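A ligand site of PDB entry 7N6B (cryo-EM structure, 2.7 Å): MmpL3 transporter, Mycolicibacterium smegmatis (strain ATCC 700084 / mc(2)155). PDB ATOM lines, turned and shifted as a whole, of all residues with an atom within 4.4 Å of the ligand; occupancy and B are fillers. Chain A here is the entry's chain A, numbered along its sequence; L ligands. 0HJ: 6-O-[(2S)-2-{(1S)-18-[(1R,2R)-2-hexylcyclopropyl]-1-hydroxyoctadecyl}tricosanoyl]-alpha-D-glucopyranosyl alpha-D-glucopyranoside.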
ATOM      1  N   LEU A 409     -21.161  33.947   7.855  1.00  0.00           N
ATOM      2  CA  LEU A 409     -21.596  32.948   8.827  1.00  0.00           C
ATOM      3  C   LEU A 409     -23.065  32.607   8.634  1.00  0.00           C
ATOM      4  O   LEU A 409     -23.451  31.422   8.653  1.00  0.00           O
ATOM      5  CB  LEU A 409     -21.353  33.469  10.246  1.00  0.00           C
ATOM      6  CG  LEU A 409     -20.072  33.051  10.991  1.00  0.00           C
ATOM      7  CD1 LEU A 409     -20.140  31.585  11.374  1.00  0.00           C
ATOM      8  CD2 LEU A 409     -18.836  33.319  10.154  1.00  0.00           C
ATOM      9  N   ILE A 416     -26.215  24.935   5.629  1.00  0.00           N
ATOM     10  CA  ILE A 416     -26.376  23.716   6.401  1.00  0.00           C
ATOM     11  C   ILE A 416     -27.846  23.335   6.506  1.00  0.00           C
ATOM     12  O   ILE A 416     -28.179  22.163   6.676  1.00  0.00           O
ATOM     13  CB  ILE A 416     -25.764  23.880   7.810  1.00  0.00           C
ATOM     14  CG1 ILE A 416     -24.299  24.302   7.710  1.00  0.00           C
ATOM     15  CG2 ILE A 416     -25.845  22.581   8.593  1.00  0.00           C
ATOM     16  CD1 ILE A 416     -23.592  24.289   9.039  1.00  0.00           C
ATOM     17  N   LEU A 419     -29.456  20.201   5.009  1.00  0.00           N
ATOM     18  CA  LEU A 419     -28.956  18.907   5.454  1.00  0.00           C
ATOM     19  C   LEU A 419     -29.990  18.106   6.236  1.00  0.00           C
ATOM     20  O   LEU A 419     -29.783  16.915   6.456  1.00  0.00           O
ATOM     21  CB  LEU A 419     -27.697  19.096   6.301  1.00  0.00           C
ATOM     22  CG  LEU A 419     -26.828  17.860   6.517  1.00  0.00           C
ATOM     23  CD1 LEU A 419     -26.377  17.320   5.184  1.00  0.00           C
ATOM     24  CD2 LEU A 419     -25.638  18.192   7.392  1.00  0.00           C
ATOM     25  N   GLY A 420     -31.103  18.727   6.635  1.00  0.00           N
ATOM     26  CA  GLY A 420     -32.105  18.014   7.386  1.00  0.00           C
ATOM     27  C   GLY A 420     -32.939  17.050   6.586  1.00  0.00           C
ATOM     28  O   GLY A 420     -33.676  16.247   7.165  1.00  0.00           O
ATOM     29  N   LEU A 422     -31.475  14.930   4.371  1.00  0.00           N
ATOM     30  CA  LEU A 422     -30.585  13.887   3.893  1.00  0.00           C
ATOM     31  C   LEU A 422     -31.146  12.517   4.275  1.00  0.00           C
ATOM     32  O   LEU A 422     -31.554  12.302   5.421  1.00  0.00           O
ATOM     33  CB  LEU A 422     -29.181  14.081   4.479  1.00  0.00           C
ATOM     34  CG  LEU A 422     -28.032  13.196   3.969  1.00  0.00           C
ATOM     35  CD1 LEU A 422     -26.709  13.921   4.122  1.00  0.00           C
ATOM     36  CD2 LEU A 422     -27.963  11.895   4.725  1.00  0.00           C
ATOM     37  N   SER A 423     -31.157  11.610   3.310  1.00  0.00           N
ATOM     38  CA  SER A 423     -31.620  10.247   3.522  1.00  0.00           C
ATOM     39  C   SER A 423     -30.535   9.280   3.074  1.00  0.00           C
ATOM     40  O   SER A 423     -29.767   9.572   2.156  1.00  0.00           O
ATOM     41  CB  SER A 423     -32.922   9.965   2.755  1.00  0.00           C
ATOM     42  OG  SER A 423     -32.740  10.171   1.363  1.00  0.00           O
ATOM     43  N   LEU A 424     -30.482   8.126   3.737  1.00  0.00           N
ATOM     44  CA  LEU A 424     -29.444   7.148   3.475  1.00  0.00           C
ATOM     45  C   LEU A 424     -30.034   5.999   2.662  1.00  0.00           C
ATOM     46  O   LEU A 424     -31.216   5.662   2.819  1.00  0.00           O
ATOM     47  CB  LEU A 424     -28.856   6.594   4.778  1.00  0.00           C
ATOM     48  CG  LEU A 424     -27.820   7.429   5.526  1.00  0.00           C
ATOM     49  CD1 LEU A 424     -26.581   7.688   4.691  1.00  0.00           C
ATOM     50  CD2 LEU A 424     -28.403   8.726   6.074  1.00  0.00           C
ATOM     51  N   PHE A 561     -24.263   4.991  11.787  1.00  0.00           N
ATOM     52  CA  PHE A 561     -24.857   5.933  12.722  1.00  0.00           C
ATOM     53  C   PHE A 561     -24.352   5.715  14.135  1.00  0.00           C
ATOM     54  O   PHE A 561     -24.128   6.686  14.875  1.00  0.00           O
ATOM     55  CB  PHE A 561     -26.380   5.839  12.688  1.00  0.00           C
ATOM     56  CG  PHE A 561     -27.012   6.618  11.581  1.00  0.00           C
ATOM     57  CD1 PHE A 561     -26.274   7.517  10.836  1.00  0.00           C
ATOM     58  CD2 PHE A 561     -28.363   6.476  11.300  1.00  0.00           C
ATOM     59  CE1 PHE A 561     -26.856   8.242   9.813  1.00  0.00           C
ATOM     60  CE2 PHE A 561     -28.956   7.199  10.284  1.00  0.00           C
ATOM     61  CZ  PHE A 561     -28.192   8.084   9.538  1.00  0.00           C
ATOM     62  N   LEU A 564     -20.602   7.083  14.386  1.00  0.00           N
ATOM     63  CA  LEU A 564     -20.316   8.388  13.811  1.00  0.00           C
ATOM     64  C   LEU A 564     -19.942   9.433  14.873  1.00  0.00           C
ATOM     65  O   LEU A 564     -19.018  10.227  14.625  1.00  0.00           O
ATOM     66  CB  LEU A 564     -21.506   8.868  12.972  1.00  0.00           C
ATOM     67  CG  LEU A 564     -21.318  10.190  12.251  1.00  0.00           C
ATOM     68  CD1 LEU A 564     -20.188  10.077  11.251  1.00  0.00           C
ATOM     69  CD2 LEU A 564     -22.602  10.607  11.558  1.00  0.00           C
ATOM     70  N   ALA A 568     -16.518  11.680  14.898  1.00  0.00           N
ATOM     71  CA  ALA A 568     -16.444  13.124  15.011  1.00  0.00           C
ATOM     72  C   ALA A 568     -15.519  13.542  16.143  1.00  0.00           C
ATOM     73  O   ALA A 568     -14.711  14.469  15.995  1.00  0.00           O
ATOM     74  CB  ALA A 568     -17.838  13.712  15.234  1.00  0.00           C
ATOM     75  N   ILE A 572     -12.117  15.723  15.569  1.00  0.00           N
ATOM     76  CA  ILE A 572     -11.906  17.033  16.157  1.00  0.00           C
ATOM     77  C   ILE A 572     -10.666  17.031  17.038  1.00  0.00           C
ATOM     78  O   ILE A 572      -9.799  17.904  16.902  1.00  0.00           O
ATOM     79  CB  ILE A 572     -13.149  17.483  16.933  1.00  0.00           C
ATOM     80  CG1 ILE A 572     -14.296  17.783  15.967  1.00  0.00           C
ATOM     81  CG2 ILE A 572     -12.846  18.702  17.788  1.00  0.00           C
ATOM     82  CD1 ILE A 572     -15.669  17.574  16.547  1.00  0.00           C
ATOM     83  N   VAL A 573     -10.532  16.038  17.920  1.00  0.00           N
ATOM     84  CA  VAL A 573      -9.444  16.061  18.889  1.00  0.00           C
ATOM     85  C   VAL A 573      -8.095  15.901  18.191  1.00  0.00           C
ATOM     86  O   VAL A 573      -7.151  16.658  18.446  1.00  0.00           O
ATOM     87  CB  VAL A 573      -9.663  14.988  19.965  1.00  0.00           C
ATOM     88  CG1 VAL A 573      -8.480  14.948  20.906  1.00  0.00           C
ATOM     89  CG2 VAL A 573     -10.936  15.280  20.736  1.00  0.00           C
ATOM     90  N   THR A 576      -7.285  19.025  16.014  1.00  0.00           N
ATOM     91  CA  THR A 576      -6.977  20.229  16.788  1.00  0.00           C
ATOM     92  C   THR A 576      -5.633  20.099  17.493  1.00  0.00           C
ATOM     93  O   THR A 576      -4.891  21.084  17.591  1.00  0.00           O
ATOM     94  CB  THR A 576      -8.112  20.528  17.768  1.00  0.00           C
ATOM     95  OG1 THR A 576      -7.956  21.853  18.296  1.00  0.00           O
ATOM     96  CG2 THR A 576      -8.120  19.558  18.941  1.00  0.00           C
ATOM     97  N   ILE A 590      -8.875  25.751  17.587  1.00  0.00           N
ATOM     98  CA  ILE A 590     -10.326  25.843  17.694  1.00  0.00           C
ATOM     99  C   ILE A 590     -10.901  26.750  16.612  1.00  0.00           C
ATOM    100  O   ILE A 590     -11.951  26.451  16.028  1.00  0.00           O
ATOM    101  CB  ILE A 590     -10.781  26.279  19.098  1.00  0.00           C
ATOM    102  CG1 ILE A 590     -10.387  25.226  20.149  1.00  0.00           C
ATOM    103  CG2 ILE A 590     -12.265  26.549  19.135  1.00  0.00           C
ATOM    104  CD1 ILE A 590      -9.053  25.383  20.759  1.00  0.00           C
ATOM    105  N   ALA A 593     -10.897  24.616  13.504  1.00  0.00           N
ATOM    106  CA  ALA A 593     -11.847  23.519  13.594  1.00  0.00           C
ATOM    107  C   ALA A 593     -13.278  23.994  13.449  1.00  0.00           C
ATOM    108  O   ALA A 593     -14.098  23.322  12.825  1.00  0.00           O
ATOM    109  CB  ALA A 593     -11.668  22.772  14.918  1.00  0.00           C
ATOM    110  N   LEU A 594     -13.612  25.158  14.022  1.00  0.00           N
ATOM    111  CA  LEU A 594     -14.960  25.705  13.843  1.00  0.00           C
ATOM    112  C   LEU A 594     -15.232  26.015  12.376  1.00  0.00           C
ATOM    113  O   LEU A 594     -16.326  25.718  11.873  1.00  0.00           O
ATOM    114  CB  LEU A 594     -15.139  26.950  14.707  1.00  0.00           C
ATOM    115  CG  LEU A 594     -15.101  26.714  16.211  1.00  0.00           C
ATOM    116  CD1 LEU A 594     -15.210  28.033  16.963  1.00  0.00           C
ATOM    117  CD2 LEU A 594     -16.193  25.756  16.644  1.00  0.00           C
ATOM    118  N   ALA A 597     -15.693  22.764  10.505  1.00  0.00           N
ATOM    119  CA  ALA A 597     -17.046  22.254  10.752  1.00  0.00           C
ATOM    120  C   ALA A 597     -18.080  23.020   9.934  1.00  0.00           C
ATOM    121  O   ALA A 597     -18.994  22.414   9.368  1.00  0.00           O
ATOM    122  CB  ALA A 597     -17.369  22.342  12.241  1.00  0.00           C
ATOM    123  N   LEU A 598     -17.948  24.342   9.867  1.00  0.00           N
ATOM    124  CA  LEU A 598     -18.881  25.142   9.075  1.00  0.00           C
ATOM    125  C   LEU A 598     -18.786  24.796   7.595  1.00  0.00           C
ATOM    126  O   LEU A 598     -19.804  24.668   6.910  1.00  0.00           O
ATOM    127  CB  LEU A 598     -18.621  26.622   9.304  1.00  0.00           C
ATOM    128  CG  LEU A 598     -19.678  27.596   8.784  1.00  0.00           C
ATOM    129  CD1 LEU A 598     -20.979  27.406   9.520  1.00  0.00           C
ATOM    130  CD2 LEU A 598     -19.176  29.015   8.925  1.00  0.00           C
ATOM    131  N   LEU A 600     -17.710  21.957   6.297  1.00  0.00           N
ATOM    132  CA  LEU A 600     -18.267  20.623   6.131  1.00  0.00           C
ATOM    133  C   LEU A 600     -19.789  20.662   6.127  1.00  0.00           C
ATOM    134  O   LEU A 600     -20.433  20.023   5.290  1.00  0.00           O
ATOM    135  CB  LEU A 600     -17.755  19.713   7.246  1.00  0.00           C
ATOM    136  CG  LEU A 600     -18.208  18.256   7.218  1.00  0.00           C
ATOM    137  CD1 LEU A 600     -17.496  17.518   6.110  1.00  0.00           C
ATOM    138  CD2 LEU A 600     -17.944  17.601   8.558  1.00  0.00           C
ATOM    139  N   GLY A 601     -20.391  21.409   7.057  1.00  0.00           N
ATOM    140  CA  GLY A 601     -21.836  21.494   7.114  1.00  0.00           C
ATOM    141  C   GLY A 601     -22.428  22.110   5.867  1.00  0.00           C
ATOM    142  O   GLY A 601     -23.419  21.613   5.320  1.00  0.00           O
ATOM    143  N   MET A 604     -22.047  19.620   2.918  1.00  0.00           N
ATOM    144  CA  MET A 604     -23.021  18.541   3.031  1.00  0.00           C
ATOM    145  C   MET A 604     -24.426  19.045   2.713  1.00  0.00           C
ATOM    146  O   MET A 604     -25.234  18.318   2.118  1.00  0.00           O
ATOM    147  CB  MET A 604     -22.964  17.931   4.430  1.00  0.00           C
ATOM    148  CG  MET A 604     -21.658  17.215   4.739  1.00  0.00           C
ATOM    149  SD  MET A 604     -21.343  15.837   3.624  1.00  0.00           S
ATOM    150  CE  MET A 604     -22.618  14.695   4.166  1.00  0.00           C
ATOM    151  N   ILE A 632     -20.899   8.632   3.482  1.00  0.00           N
ATOM    152  CA  ILE A 632     -21.104   9.845   4.278  1.00  0.00           C
ATOM    153  C   ILE A 632     -19.876  10.103   5.150  1.00  0.00           C
ATOM    154  O   ILE A 632     -19.308  11.205   5.132  1.00  0.00           O
ATOM    155  CB  ILE A 632     -22.373   9.719   5.133  1.00  0.00           C
ATOM    156  CG1 ILE A 632     -23.618   9.912   4.263  1.00  0.00           C
ATOM    157  CG2 ILE A 632     -22.358  10.733   6.267  1.00  0.00           C
ATOM    158  CD1 ILE A 632     -23.652  11.242   3.547  1.00  0.00           C
ATOM    159  N   ILE A 636     -17.078  13.072   4.768  1.00  0.00           N
ATOM    160  CA  ILE A 636     -16.834  13.890   5.959  1.00  0.00           C
ATOM    161  C   ILE A 636     -15.337  13.951   6.251  1.00  0.00           C
ATOM    162  O   ILE A 636     -14.757  15.037   6.416  1.00  0.00           O
ATOM    163  CB  ILE A 636     -17.607  13.332   7.164  1.00  0.00           C
ATOM    164  CG1 ILE A 636     -19.085  13.686   7.069  1.00  0.00           C
ATOM    165  CG2 ILE A 636     -17.025  13.849   8.467  1.00  0.00           C
ATOM    166  CD1 ILE A 636     -19.935  13.009   8.105  1.00  0.00           C
HETATM  167  C10 0HJ L   1     -29.788  14.169   9.576  1.00  0.00           C
HETATM  168  C21 0HJ L   1     -26.567  12.122   9.273  1.00  0.00           C
HETATM  169  C24 0HJ L   1     -24.538  13.345   9.361  1.00  0.00           C
HETATM  170  C26 0HJ L   1     -23.490  14.310   9.932  1.00  0.00           C
HETATM  171  C28 0HJ L   1     -22.116  16.347   9.480  1.00  0.00           C
HETATM  172  C01 0HJ L   1     -33.187   8.031   9.023  1.00  0.00           C
HETATM  173  C02 0HJ L   1     -33.982   9.170   9.469  1.00  0.00           C
HETATM  174  C03 0HJ L   1     -33.178  10.335   9.915  1.00  0.00           C
HETATM  175  C04 0HJ L   1     -31.992  10.722   8.946  1.00  0.00           C
HETATM  176  C06 0HJ L   1     -32.172   8.373   7.975  1.00  0.00           C
HETATM  177  C08 0HJ L   1     -30.009  11.774   9.552  1.00  0.00           C
HETATM  178  C09 0HJ L   1     -30.659  13.065   9.219  1.00  0.00           C
HETATM  179  C11 0HJ L   1     -28.388  13.750   9.842  1.00  0.00           C
HETATM  180  C12 0HJ L   1     -27.809  12.694   8.830  1.00  0.00           C
HETATM  181  C14 0HJ L   1     -32.601   7.692   6.683  1.00  0.00           C
HETATM  182  C27 0HJ L   1     -23.180  15.392   8.872  1.00  0.00           C
HETATM  183  C29 0HJ L   1     -22.352  17.790   8.954  1.00  0.00           C
HETATM  184  C30 0HJ L   1     -21.493  18.788   9.779  1.00  0.00           C
HETATM  185  C31 0HJ L   1     -22.460  19.743  10.537  1.00  0.00           C
HETATM  186  C32 0HJ L   1     -21.645  20.805  11.322  1.00  0.00           C
HETATM  187  C33 0HJ L   1     -22.570  22.017  11.627  1.00  0.00           C
HETATM  188  C34 0HJ L   1     -22.272  22.575  13.038  1.00  0.00           C
HETATM  189  C35 0HJ L   1     -22.006  24.098  12.982  1.00  0.00           C
HETATM  190  C36 0HJ L   1     -20.517  24.339  12.665  1.00  0.00           C
HETATM  191  C37 0HJ L   1     -20.013  25.571  13.444  1.00  0.00           C
HETATM  192  C38 0HJ L   1     -20.939  26.753  13.143  1.00  0.00           C
HETATM  193  C39 0HJ L   1     -20.128  28.077  13.072  1.00  0.00           C
HETATM  194  C40 0HJ L   1     -19.672  28.533  14.478  1.00  0.00           C
HETATM  195  C43 0HJ L   1     -23.938  15.001  11.220  1.00  0.00           C
HETATM  196  C45 0HJ L   1     -23.903  14.031  12.437  1.00  0.00           C
HETATM  197  C46 0HJ L   1     -22.972  14.557  13.571  1.00  0.00           C
HETATM  198  C47 0HJ L   1     -21.777  13.593  13.807  1.00  0.00           C
HETATM  199  C48 0HJ L   1     -20.569  13.989  12.908  1.00  0.00           C
HETATM  200  C49 0HJ L   1     -20.204  15.505  13.103  1.00  0.00           C
HETATM  201  C50 0HJ L   1     -19.277  16.000  11.940  1.00  0.00           C
HETATM  202  C51 0HJ L   1     -18.037  16.784  12.482  1.00  0.00           C
HETATM  203  C52 0HJ L   1     -18.491  17.641  13.699  1.00  0.00           C
HETATM  204  C53 0HJ L   1     -18.935  19.036  13.198  1.00  0.00           C
HETATM  205  C54 0HJ L   1     -19.695  19.787  14.343  1.00  0.00           C
HETATM  206  C55 0HJ L   1     -19.102  19.432  15.733  1.00  0.00           C
HETATM  207  C56 0HJ L   1     -18.519  20.711  16.405  1.00  0.00           C
HETATM  208  C57 0HJ L   1     -17.068  20.994  15.927  1.00  0.00           C
HETATM  209  C58 0HJ L   1     -16.262  21.548  17.125  1.00  0.00           C
HETATM  210  C59 0HJ L   1     -14.863  21.970  16.617  1.00  0.00           C
HETATM  211  C60 0HJ L   1     -13.844  22.198  17.776  1.00  0.00           C
HETATM  212  C61 0HJ L   1     -14.459  22.895  19.023  1.00  0.00           C
HETATM  213  C67 0HJ L   1     -13.906  22.149  20.260  1.00  0.00           C
HETATM  214  C68 0HJ L   1     -12.378  22.071  20.333  1.00  0.00           C
HETATM  215  C69 0HJ L   1     -11.821  20.728  20.874  1.00  0.00           C
HETATM  216  C70 0HJ L   1     -10.405  20.907  21.475  1.00  0.00           C
HETATM  217  C71 0HJ L   1     -13.142  22.960  21.316  1.00  0.00           C
HETATM  218  O05 0HJ L   1     -32.051   9.823   7.704  1.00  0.00           O
HETATM  219  O07 0HJ L   1     -30.839  10.598   9.540  1.00  0.00           O
HETATM  220  O13 0HJ L   1     -28.835  11.560   8.680  1.00  0.00           O
HETATM  221  O15 0HJ L   1     -31.635   6.742   6.292  1.00  0.00           O
HETATM  222  O16 0HJ L   1     -32.502   7.437  10.181  1.00  0.00           O
HETATM  223  O17 0HJ L   1     -34.866   9.585   8.352  1.00  0.00           O
HETATM  224  O18 0HJ L   1     -30.843  13.221   7.752  1.00  0.00           O
HETATM  225  O19 0HJ L   1     -30.319  14.843  10.787  1.00  0.00           O
HETATM  226  O20 0HJ L   1     -27.613  14.957   9.772  1.00  0.00           O
HETATM  227  O22 0HJ L   1     -32.635  10.074  11.207  1.00  0.00           O
HETATM  228  O23 0HJ L   1     -25.768  13.052  10.002  1.00  0.00           O
HETATM  229  O25 0HJ L   1     -24.292  12.811   8.333  1.00  0.00           O
HETATM  230  O44 0HJ L   1     -25.226  15.502  11.042  1.00  0.00           O
HETATM  231  C1  0HJ L   1      -9.912  19.518  21.990  1.00  0.00           C
HETATM  232  C2  0HJ L   1      -8.633  19.673  22.847  1.00  0.00           C
HETATM  233  C3  0HJ L   1      -8.198  18.274  23.345  1.00  0.00           C
HETATM  234  C4  0HJ L   1      -7.235  18.432  24.557  1.00  0.00           C
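O of Leu 422 lies within hydrogen-bond range of O18 of the ligand.
The backbone NH (N) of Leu 424 is in hydrogen-bond range of an oxygen (O15) of the ligand (3.1 Å).
CD1 of Leu 409 touches C39 of the ligand (3.9 Å).
Ile 416 touches the ligand (CD1 to C33, 3.6 Å).
CD2 of Leu 419 touches C29 of the ligand, 3.7 Å away.
CE2 of Phe 561 touches O16 of the ligand, 3.6 Å away.
Leu 564 touches the ligand.
Ala 568 touches the ligand (CB to C48, 3.6 Å).
Ile 572 touches the ligand.
Thr 576 touches the ligand.
Ile 590 touches the ligand.
Ala 593 touches the ligand (CB to C60, 3.6 Å).
Ala 597 touches the ligand.
CD1 of Leu 598 touches C38 of the ligand, 3.7 Å away.
Leu 600 touches the ligand.
CA of Gly 601 touches C30 of the ligand, 3.8 Å away.
Ile 632 touches the ligand.
Hydrophobic or aromatic side chains that line the ligand: Leu 409, Ile 416, Leu 419, Leu 422, Leu 424, Phe 561, Leu 564, Ala 568, Ile 572, Ile 590, Ala 593, Ala 597, Leu 598, Leu 600 and Ile 632.
The nearest printed residue that does not touch the ligand is Leu 594 (4.01 Å).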
